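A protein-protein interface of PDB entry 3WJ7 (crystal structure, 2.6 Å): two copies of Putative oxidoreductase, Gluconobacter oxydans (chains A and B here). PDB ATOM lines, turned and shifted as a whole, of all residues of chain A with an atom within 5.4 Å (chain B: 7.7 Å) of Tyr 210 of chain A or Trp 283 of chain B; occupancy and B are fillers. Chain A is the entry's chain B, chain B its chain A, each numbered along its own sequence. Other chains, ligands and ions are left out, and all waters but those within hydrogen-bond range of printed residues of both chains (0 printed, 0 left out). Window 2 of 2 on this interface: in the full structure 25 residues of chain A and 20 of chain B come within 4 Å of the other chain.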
ATOM      1  N   MET A 198      18.963 -12.605   6.083  1.00  0.00           N
ATOM      2  CA  MET A 198      20.154 -11.786   6.238  1.00  0.00           C
ATOM      3  C   MET A 198      20.803 -11.577   4.891  1.00  0.00           C
ATOM      4  O   MET A 198      21.169 -10.459   4.573  1.00  0.00           O
ATOM      5  CB  MET A 198      21.165 -12.385   7.192  1.00  0.00           C
ATOM      6  CG  MET A 198      20.876 -12.155   8.661  1.00  0.00           C
ATOM      7  SD  MET A 198      21.787 -13.373   9.647  1.00  0.00           S
ATOM      8  CE  MET A 198      23.182 -12.467  10.256  1.00  0.00           C
ATOM      9  N   MET A 207      20.407  -3.487   6.314  1.00  0.00           N
ATOM     10  CA  MET A 207      20.906  -4.139   7.521  1.00  0.00           C
ATOM     11  C   MET A 207      21.920  -3.092   7.878  1.00  0.00           C
ATOM     12  O   MET A 207      23.008  -3.065   7.305  1.00  0.00           O
ATOM     13  CB  MET A 207      21.640  -5.454   7.189  1.00  0.00           C
ATOM     14  CG  MET A 207      21.738  -6.551   8.247  1.00  0.00           C
ATOM     15  SD  MET A 207      22.374  -8.047   7.421  1.00  0.00           S
ATOM     16  CE  MET A 207      23.953  -7.248   7.113  1.00  0.00           C
ATOM     17  N   PRO A 208      21.553  -2.168   8.768  1.00  0.00           N
ATOM     18  CA  PRO A 208      22.556  -1.156   9.100  1.00  0.00           C
ATOM     19  C   PRO A 208      23.592  -1.691  10.139  1.00  0.00           C
ATOM     20  O   PRO A 208      24.774  -1.341  10.091  1.00  0.00           O
ATOM     21  CB  PRO A 208      21.700  -0.004   9.644  1.00  0.00           C
ATOM     22  CG  PRO A 208      20.444  -0.664  10.184  1.00  0.00           C
ATOM     23  CD  PRO A 208      20.303  -2.018   9.544  1.00  0.00           C
ATOM     24  N   ALA A 209      23.147  -2.566  11.036  1.00  0.00           N
ATOM     25  CA  ALA A 209      24.015  -3.156  12.048  1.00  0.00           C
ATOM     26  C   ALA A 209      23.961  -4.700  12.045  1.00  0.00           C
ATOM     27  O   ALA A 209      23.053  -5.307  11.448  1.00  0.00           O
ATOM     28  CB  ALA A 209      23.649  -2.605  13.415  1.00  0.00           C
ATOM     29  N   TYR A 210      24.958  -5.321  12.686  1.00  0.00           N
ATOM     30  CA  TYR A 210      24.931  -6.762  12.991  1.00  0.00           C
ATOM     31  C   TYR A 210      25.837  -7.010  14.193  1.00  0.00           C
ATOM     32  O   TYR A 210      26.747  -6.221  14.404  1.00  0.00           O
ATOM     33  CB  TYR A 210      25.424  -7.578  11.796  1.00  0.00           C
ATOM     34  CG  TYR A 210      26.875  -7.335  11.460  1.00  0.00           C
ATOM     35  CD1 TYR A 210      27.871  -8.091  12.022  1.00  0.00           C
ATOM     36  CD2 TYR A 210      27.247  -6.327  10.567  1.00  0.00           C
ATOM     37  CE1 TYR A 210      29.188  -7.867  11.700  1.00  0.00           C
ATOM     38  CE2 TYR A 210      28.585  -6.102  10.236  1.00  0.00           C
ATOM     39  CZ  TYR A 210      29.544  -6.870  10.812  1.00  0.00           C
ATOM     40  OH  TYR A 210      30.881  -6.633  10.517  1.00  0.00           O
ATOM     41  N   VAL A 211      25.579  -8.079  14.967  1.00  0.00           N
ATOM     42  CA  VAL A 211      26.454  -8.525  16.054  1.00  0.00           C
ATOM     43  C   VAL A 211      27.499  -9.489  15.498  1.00  0.00           C
ATOM     44  O   VAL A 211      27.129 -10.476  14.876  1.00  0.00           O
ATOM     45  CB  VAL A 211      25.700  -9.340  17.119  1.00  0.00           C
ATOM     46  CG1 VAL A 211      26.546  -9.467  18.391  1.00  0.00           C
ATOM     47  CG2 VAL A 211      24.312  -8.763  17.398  1.00  0.00           C
ATOM     48  N   GLU A 212      28.786  -9.225  15.711  1.00  0.00           N
ATOM     49  CA  GLU A 212      29.804 -10.150  15.224  1.00  0.00           C
ATOM     50  C   GLU A 212      29.623 -11.540  15.862  1.00  0.00           C
ATOM     51  O   GLU A 212      29.355 -11.673  17.078  1.00  0.00           O
ATOM     52  CB  GLU A 212      31.238  -9.625  15.427  1.00  0.00           C
ATOM     53  CG  GLU A 212      32.367 -10.409  14.678  1.00  0.00           C
ATOM     54  CD  GLU A 212      32.251 -10.486  13.128  1.00  0.00           C
ATOM     55  OE1 GLU A 212      31.160 -10.694  12.610  1.00  0.00           O
ATOM     56  OE2 GLU A 212      33.258 -10.373  12.402  1.00  0.00           O
ATOM     57  N   LEU A 249      30.892 -13.302  10.614  1.00  0.00           N
ATOM     58  CA  LEU A 249      29.673 -12.728  10.056  1.00  0.00           C
ATOM     59  C   LEU A 249      29.931 -11.421   9.240  1.00  0.00           C
ATOM     60  O   LEU A 249      29.327 -11.174   8.190  1.00  0.00           O
ATOM     61  CB  LEU A 249      28.680 -12.517  11.174  1.00  0.00           C
ATOM     62  CG  LEU A 249      27.224 -12.376  10.680  1.00  0.00           C
ATOM     63  CD1 LEU A 249      26.660 -13.626   9.953  1.00  0.00           C
ATOM     64  CD2 LEU A 249      26.341 -12.000  11.868  1.00  0.00           C
ATOM     65  N   GLY A 250      30.836 -10.583   9.712  1.00  0.00           N
ATOM     66  CA  GLY A 250      31.193  -9.407   8.992  1.00  0.00           C
ATOM     67  C   GLY A 250      31.861  -9.766   7.680  1.00  0.00           C
ATOM     68  O   GLY A 250      31.607  -9.120   6.678  1.00  0.00           O
ATOM     69  N   ASP A 251      32.693 -10.807   7.655  1.00  0.00           N
ATOM     70  CA  ASP A 251      33.227 -11.257   6.372  1.00  0.00           C
ATOM     71  C   ASP A 251      32.150 -11.798   5.439  1.00  0.00           C
ATOM     72  O   ASP A 251      32.199 -11.552   4.260  1.00  0.00           O
ATOM     73  CB  ASP A 251      34.389 -12.223   6.533  1.00  0.00           C
ATOM     74  CG  ASP A 251      35.539 -11.603   7.283  1.00  0.00           C
ATOM     75  OD1 ASP A 251      35.872 -10.422   7.020  1.00  0.00           O
ATOM     76  OD2 ASP A 251      36.107 -12.280   8.172  1.00  0.00           O
ATOM     77  N   PHE A 253      29.023 -10.771   5.312  1.00  0.00           N
ATOM     78  CA  PHE A 253      28.364  -9.552   4.820  1.00  0.00           C
ATOM     79  C   PHE A 253      29.208  -8.711   3.855  1.00  0.00           C
ATOM     80  O   PHE A 253      28.709  -8.207   2.854  1.00  0.00           O
ATOM     81  CB  PHE A 253      27.911  -8.705   6.002  1.00  0.00           C
ATOM     82  CG  PHE A 253      26.800  -9.329   6.807  1.00  0.00           C
ATOM     83  CD1 PHE A 253      26.552  -8.904   8.112  1.00  0.00           C
ATOM     84  CD2 PHE A 253      25.998 -10.350   6.265  1.00  0.00           C
ATOM     85  CE1 PHE A 253      25.503  -9.460   8.857  1.00  0.00           C
ATOM     86  CE2 PHE A 253      24.992 -10.918   7.012  1.00  0.00           C
ATOM     87  CZ  PHE A 253      24.725 -10.461   8.312  1.00  0.00           C
ATOM     88  N   ARG A 254      30.494  -8.576   4.128  1.00  0.00           N
ATOM     89  CA  ARG A 254      31.350  -7.897   3.160  1.00  0.00           C
ATOM     90  C   ARG A 254      31.281  -8.671   1.827  1.00  0.00           C
ATOM     91  O   ARG A 254      31.149  -8.069   0.758  1.00  0.00           O
ATOM     92  CB  ARG A 254      32.784  -7.685   3.672  1.00  0.00           C
ATOM     93  CG  ARG A 254      33.022  -6.285   4.230  1.00  0.00           C
ATOM     94  CD  ARG A 254      34.318  -6.135   5.050  1.00  0.00           C
ATOM     95  NE  ARG A 254      34.099  -6.685   6.378  1.00  0.00           N
ATOM     96  CZ  ARG A 254      34.846  -6.478   7.455  1.00  0.00           C
ATOM     97  NH1 ARG A 254      35.917  -5.691   7.410  1.00  0.00           N
ATOM     98  NH2 ARG A 254      34.504  -7.076   8.590  1.00  0.00           N
ATOM     99  N   PRO A 265      27.647  -3.372   5.491  1.00  0.00           N
ATOM    100  CA  PRO A 265      27.207  -2.616   6.682  1.00  0.00           C
ATOM    101  C   PRO A 265      28.429  -2.154   7.446  1.00  0.00           C
ATOM    102  O   PRO A 265      29.477  -2.811   7.414  1.00  0.00           O
ATOM    103  CB  PRO A 265      26.428  -3.645   7.521  1.00  0.00           C
ATOM    104  CG  PRO A 265      26.896  -4.987   7.048  1.00  0.00           C
ATOM    105  CD  PRO A 265      27.610  -4.835   5.709  1.00  0.00           C
ATOM    106  N   VAL A 267      28.291  -0.864  10.818  1.00  0.00           N
ATOM    107  CA  VAL A 267      28.099  -0.903  12.260  1.00  0.00           C
ATOM    108  C   VAL A 267      28.180  -2.336  12.761  1.00  0.00           C
ATOM    109  O   VAL A 267      27.196  -3.067  12.726  1.00  0.00           O
ATOM    110  CB  VAL A 267      26.746  -0.335  12.631  1.00  0.00           C
ATOM    111  CG1 VAL A 267      26.574  -0.314  14.127  1.00  0.00           C
ATOM    112  CG2 VAL A 267      26.615   1.052  12.043  1.00  0.00           C
ATOM    113  N   LYS A 268      29.369  -2.715  13.207  1.00  0.00           N
ATOM    114  CA  LYS A 268      29.641  -4.018  13.738  1.00  0.00           C
ATOM    115  C   LYS A 268      29.648  -3.944  15.250  1.00  0.00           C
ATOM    116  O   LYS A 268      30.530  -3.293  15.824  1.00  0.00           O
ATOM    117  CB  LYS A 268      31.002  -4.483  13.216  1.00  0.00           C
ATOM    118  CG  LYS A 268      31.641  -5.542  14.062  1.00  0.00           C
ATOM    119  CD  LYS A 268      32.813  -6.125  13.315  1.00  0.00           C
ATOM    120  CE  LYS A 268      33.912  -6.466  14.289  1.00  0.00           C
ATOM    121  NZ  LYS A 268      34.795  -7.458  13.628  1.00  0.00           N
ATOM    122  N   LEU A 269      28.683  -4.615  15.887  1.00  0.00           N
ATOM    123  CA  LEU A 269      28.585  -4.687  17.349  1.00  0.00           C
ATOM    124  C   LEU A 269      29.351  -5.896  17.961  1.00  0.00           C
ATOM    125  O   LEU A 269      29.014  -7.066  17.678  1.00  0.00           O
ATOM    126  CB  LEU A 269      27.118  -4.795  17.720  1.00  0.00           C
ATOM    127  CG  LEU A 269      26.122  -3.789  17.098  1.00  0.00           C
ATOM    128  CD1 LEU A 269      24.689  -4.066  17.569  1.00  0.00           C
ATOM    129  CD2 LEU A 269      26.541  -2.353  17.425  1.00  0.00           C
ATOM    130  N   PRO B 276      11.694  -0.779  14.399  1.00  0.00           N
ATOM    131  CA  PRO B 276      13.017  -0.768  15.031  1.00  0.00           C
ATOM    132  C   PRO B 276      13.158  -1.682  16.239  1.00  0.00           C
ATOM    133  O   PRO B 276      14.237  -2.270  16.422  1.00  0.00           O
ATOM    134  CB  PRO B 276      13.173   0.686  15.471  1.00  0.00           C
ATOM    135  CG  PRO B 276      12.464   1.426  14.396  1.00  0.00           C
ATOM    136  CD  PRO B 276      11.227   0.595  14.119  1.00  0.00           C
ATOM    137  N   VAL B 277      12.106  -1.783  17.059  1.00  0.00           N
ATOM    138  CA  VAL B 277      12.122  -2.631  18.255  1.00  0.00           C
ATOM    139  C   VAL B 277      12.231  -4.094  17.807  1.00  0.00           C
ATOM    140  O   VAL B 277      12.969  -4.916  18.408  1.00  0.00           O
ATOM    141  CB  VAL B 277      10.830  -2.447  19.079  1.00  0.00           C
ATOM    142  CG1 VAL B 277      10.971  -3.040  20.466  1.00  0.00           C
ATOM    143  CG2 VAL B 277      10.454  -0.975  19.175  1.00  0.00           C
ATOM    144  N   ALA B 278      11.473  -4.412  16.754  1.00  0.00           N
ATOM    145  CA  ALA B 278      11.499  -5.744  16.110  1.00  0.00           C
ATOM    146  C   ALA B 278      12.909  -6.084  15.657  1.00  0.00           C
ATOM    147  O   ALA B 278      13.426  -7.199  15.904  1.00  0.00           O
ATOM    148  CB  ALA B 278      10.570  -5.766  14.908  1.00  0.00           C
ATOM    149  N   LEU B 279      13.533  -5.098  15.014  1.00  0.00           N
ATOM    150  CA  LEU B 279      14.851  -5.268  14.502  1.00  0.00           C
ATOM    151  C   LEU B 279      15.840  -5.487  15.634  1.00  0.00           C
ATOM    152  O   LEU B 279      16.643  -6.386  15.562  1.00  0.00           O
ATOM    153  CB  LEU B 279      15.230  -4.051  13.694  1.00  0.00           C
ATOM    154  CG  LEU B 279      16.433  -4.170  12.775  1.00  0.00           C
ATOM    155  CD1 LEU B 279      16.143  -5.229  11.706  1.00  0.00           C
ATOM    156  CD2 LEU B 279      16.709  -2.780  12.189  1.00  0.00           C
ATOM    157  N   VAL B 280      15.757  -4.680  16.679  1.00  0.00           N
ATOM    158  CA  VAL B 280      16.687  -4.782  17.787  1.00  0.00           C
ATOM    159  C   VAL B 280      16.504  -6.129  18.457  1.00  0.00           C
ATOM    160  O   VAL B 280      17.472  -6.853  18.727  1.00  0.00           O
ATOM    161  CB  VAL B 280      16.501  -3.635  18.809  1.00  0.00           C
ATOM    162  CG1 VAL B 280      17.520  -3.755  19.929  1.00  0.00           C
ATOM    163  CG2 VAL B 280      16.677  -2.295  18.109  1.00  0.00           C
ATOM    164  N   SER B 281      15.253  -6.451  18.721  1.00  0.00           N
ATOM    165  CA  SER B 281      14.849  -7.785  19.159  1.00  0.00           C
ATOM    166  C   SER B 281      15.484  -8.944  18.363  1.00  0.00           C
ATOM    167  O   SER B 281      16.023  -9.850  18.958  1.00  0.00           O
ATOM    168  CB  SER B 281      13.321  -7.855  19.152  1.00  0.00           C
ATOM    169  OG  SER B 281      12.872  -9.176  19.257  1.00  0.00           O
ATOM    170  N   GLU B 282      15.449  -8.916  17.034  1.00  0.00           N
ATOM    171  CA  GLU B 282      16.144  -9.941  16.247  1.00  0.00           C
ATOM    172  C   GLU B 282      17.625  -9.912  16.505  1.00  0.00           C
ATOM    173  O   GLU B 282      18.239 -10.975  16.621  1.00  0.00           O
ATOM    174  CB  GLU B 282      15.922  -9.783  14.754  1.00  0.00           C
ATOM    175  CG  GLU B 282      14.487 -10.012  14.304  1.00  0.00           C
ATOM    176  CD  GLU B 282      14.241  -9.700  12.819  1.00  0.00           C
ATOM    177  OE1 GLU B 282      15.160  -9.882  11.972  1.00  0.00           O
ATOM    178  OE2 GLU B 282      13.096  -9.279  12.485  1.00  0.00           O
ATOM    179  N   TRP B 283      18.220  -8.724  16.609  1.00  0.00           N
ATOM    180  CA  TRP B 283      19.668  -8.680  16.863  1.00  0.00           C
ATOM    181  C   TRP B 283      20.101  -9.137  18.247  1.00  0.00           C
ATOM    182  O   TRP B 283      21.082  -9.850  18.364  1.00  0.00           O
ATOM    183  CB  TRP B 283      20.324  -7.362  16.426  1.00  0.00           C
ATOM    184  CG  TRP B 283      20.505  -7.417  14.930  1.00  0.00           C
ATOM    185  CD1 TRP B 283      19.807  -6.702  14.003  1.00  0.00           C
ATOM    186  CD2 TRP B 283      21.363  -8.321  14.176  1.00  0.00           C
ATOM    187  NE1 TRP B 283      20.188  -7.071  12.725  1.00  0.00           N
ATOM    188  CE2 TRP B 283      21.140  -8.057  12.799  1.00  0.00           C
ATOM    189  CE3 TRP B 283      22.310  -9.308  14.531  1.00  0.00           C
ATOM    190  CZ2 TRP B 283      21.828  -8.744  11.770  1.00  0.00           C
ATOM    191  CZ3 TRP B 283      23.004  -9.996  13.495  1.00  0.00           C
ATOM    192  CH2 TRP B 283      22.748  -9.705  12.142  1.00  0.00           C
ATOM    193  N   LEU B 284      19.356  -8.752  19.281  1.00  0.00           N
ATOM    194  CA  LEU B 284      19.602  -9.262  20.630  1.00  0.00           C
ATOM    195  C   LEU B 284      19.541 -10.781  20.679  1.00  0.00           C
ATOM    196  O   LEU B 284      20.530 -11.418  21.065  1.00  0.00           O
ATOM    197  CB  LEU B 284      18.657  -8.648  21.665  1.00  0.00           C
ATOM    198  CG  LEU B 284      18.923  -7.143  21.872  1.00  0.00           C
ATOM    199  CD1 LEU B 284      17.846  -6.514  22.748  1.00  0.00           C
ATOM    200  CD2 LEU B 284      20.315  -6.882  22.423  1.00  0.00           C
ATOM    201  N   ALA B 285      18.420 -11.366  20.258  1.00  0.00           N
ATOM    202  CA  ALA B 285      18.340 -12.828  20.208  1.00  0.00           C
ATOM    203  C   ALA B 285      19.479 -13.474  19.429  1.00  0.00           C
ATOM    204  O   ALA B 285      20.070 -14.446  19.932  1.00  0.00           O
ATOM    205  CB  ALA B 285      17.026 -13.294  19.677  1.00  0.00           C
ATOM    206  N   ARG B 286      19.822 -12.947  18.242  1.00  0.00           N
ATOM    207  CA  ARG B 286      20.935 -13.545  17.501  1.00  0.00           C
ATOM    208  C   ARG B 286      22.206 -13.490  18.310  1.00  0.00           C
ATOM    209  O   ARG B 286      22.871 -14.497  18.456  1.00  0.00           O
ATOM    210  CB  ARG B 286      21.162 -12.935  16.140  1.00  0.00           C
ATOM    211  CG  ARG B 286      21.906 -13.901  15.241  1.00  0.00           C
ATOM    212  CD  ARG B 286      22.021 -13.408  13.805  1.00  0.00           C
ATOM    213  NE  ARG B 286      20.793 -13.643  13.032  1.00  0.00           N
ATOM    214  CZ  ARG B 286      19.924 -12.705  12.654  1.00  0.00           C
ATOM    215  NH1 ARG B 286      20.095 -11.420  12.964  1.00  0.00           N
ATOM    216  NH2 ARG B 286      18.863 -13.063  11.948  1.00  0.00           N
ATOM    217  N   GLY B 287      22.506 -12.320  18.875  1.00  0.00           N
ATOM    218  CA  GLY B 287      23.709 -12.086  19.677  1.00  0.00           C
ATOM    219  C   GLY B 287      23.849 -12.974  20.901  1.00  0.00           C
ATOM    220  O   GLY B 287      24.979 -13.277  21.329  1.00  0.00           O
ATOM    221  N   PHE B 288      22.704 -13.407  21.430  1.00  0.00           N
ATOM    222  CA  PHE B 288      22.615 -14.228  22.627  1.00  0.00           C
ATOM    223  C   PHE B 288      22.407 -15.662  22.315  1.00  0.00           C
ATOM    224  O   PHE B 288      22.311 -16.455  23.252  1.00  0.00           O
ATOM    225  CB  PHE B 288      21.450 -13.795  23.518  1.00  0.00           C
ATOM    226  CG  PHE B 288      21.798 -12.659  24.426  1.00  0.00           C
ATOM    227  CD1 PHE B 288      22.800 -12.814  25.420  1.00  0.00           C
ATOM    228  CD2 PHE B 288      21.184 -11.419  24.283  1.00  0.00           C
ATOM    229  CE1 PHE B 288      23.138 -11.741  26.248  1.00  0.00           C
ATOM    230  CE2 PHE B 288      21.520 -10.351  25.110  1.00  0.00           C
ATOM    231  CZ  PHE B 288      22.493 -10.504  26.094  1.00  0.00           C
ATOM    232  N   GLY B 289      22.331 -16.004  21.022  1.00  0.00           N
ATOM    233  CA  GLY B 289      21.964 -17.363  20.538  1.00  0.00           C
ATOM    234  C   GLY B 289      20.629 -17.916  21.036  1.00  0.00           C
ATOM    235  O   GLY B 289      20.533 -19.101  21.322  1.00  0.00           O
ATOM    236  N   PRO B 292      14.128 -15.202  19.123  1.00  0.00           N
ATOM    237  CA  PRO B 292      13.452 -13.933  19.419  1.00  0.00           C
ATOM    238  C   PRO B 292      11.978 -14.188  19.637  1.00  0.00           C
ATOM    239  O   PRO B 292      11.428 -15.055  18.999  1.00  0.00           O
ATOM    240  CB  PRO B 292      13.686 -13.094  18.169  1.00  0.00           C
ATOM    241  CG  PRO B 292      14.093 -14.071  17.106  1.00  0.00           C
ATOM    242  CD  PRO B 292      14.655 -15.297  17.754  1.00  0.00           C
ATOM    243  N   VAL B 294       9.861 -11.845  19.137  1.00  0.00           N
ATOM    244  CA  VAL B 294       9.296 -10.867  18.237  1.00  0.00           C
ATOM    245  C   VAL B 294      10.285 -10.605  17.111  1.00  0.00           C
ATOM    246  O   VAL B 294      11.470 -10.509  17.359  1.00  0.00           O
ATOM    247  CB  VAL B 294       9.028  -9.615  19.037  1.00  0.00           C
ATOM    248  CG1 VAL B 294       9.093  -8.365  18.194  1.00  0.00           C
ATOM    249  CG2 VAL B 294       7.681  -9.743  19.706  1.00  0.00           C
ATOM    250  N   ARG B 296      10.519  -8.727  12.746  1.00  0.00           N
ATOM    251  CA  ARG B 296       9.787  -8.127  11.601  1.00  0.00           C
ATOM    252  C   ARG B 296       8.646  -8.981  11.066  1.00  0.00           C
ATOM    253  O   ARG B 296       7.557  -8.464  10.821  1.00  0.00           O
ATOM    254  CB  ARG B 296      10.718  -7.793  10.451  1.00  0.00           C
ATOM    255  CG  ARG B 296      11.768  -6.768  10.850  1.00  0.00           C
ATOM    256  CD  ARG B 296      12.831  -6.662   9.785  1.00  0.00           C
ATOM    257  NE  ARG B 296      13.593  -7.900   9.685  1.00  0.00           N
ATOM    258  CZ  ARG B 296      14.678  -8.056   8.940  1.00  0.00           C
ATOM    259  NH1 ARG B 296      15.120  -7.056   8.212  1.00  0.00           N
ATOM    260  NH2 ARG B 296      15.317  -9.220   8.942  1.00  0.00           N
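No position is printed for both chains.
CE of Met 198 of chain A touches CH2 of Trp 283 of chain B (3.4 Å).
Ala 209 of chain A touches Trp 283 of chain B.
Trp 283 of chain B touches Tyr 210 of chain A (CH2 to CB, 3.4 Å).
Trp 283 of chain B touches Val 211 of chain A (CE3 to N, 3.5 Å).
NE of Arg 286 of chain B sits at hydrogen-bond distance from SD of Met 198 of chain A (3.5 Å).
Of the 17 printed residues of chain B, 2 touch a printed residue of chain A.
Hydrophobic or aromatic side chains of chain B that line the printed part of chain A: Trp 283.
Of the 16 printed residues of chain A, 4 touch a printed residue of chain B.
Hydrophobic or aromatic side chains of chain A within 4 Å of the printed part of chain B: Met 198, Tyr 210 and Val 211.
Among the printed residues, 5 pairs touch across the chains.
The backbone NH (N) of Tyr 210 of chain A is in hydrogen-bond range of the backbone carbonyl oxygen (O) of Val 267 of chain A, 3.2 Å away.
N of Leu 269 of chain A is in hydrogen-bond range of O of Tyr 210 of chain A.
Of the printed residues of chain B, Met 198 of chain A touches Trp 283 and Arg 286.
Of the printed residues of chain B, Ala 209 of chain A touches Trp 283.
Tyr 210 of chain A touches one residue of chain B.
Printed residues of chain B within 4 Å of Val 211 of chain A: Trp 283.
Trp 283 of chain B touches just these residues of chain A: Met 198 (3.4 Å), Ala 209 (3.6 Å), Tyr 210 (3.4 Å) and Val 211 (3.5 Å).
Of the printed residues of chain A, Arg 286 of chain B touches Met 198.
The nearest residue of chain B that does not touch Tyr 210 of chain A is Arg 286 of chain B (6.7 Å).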
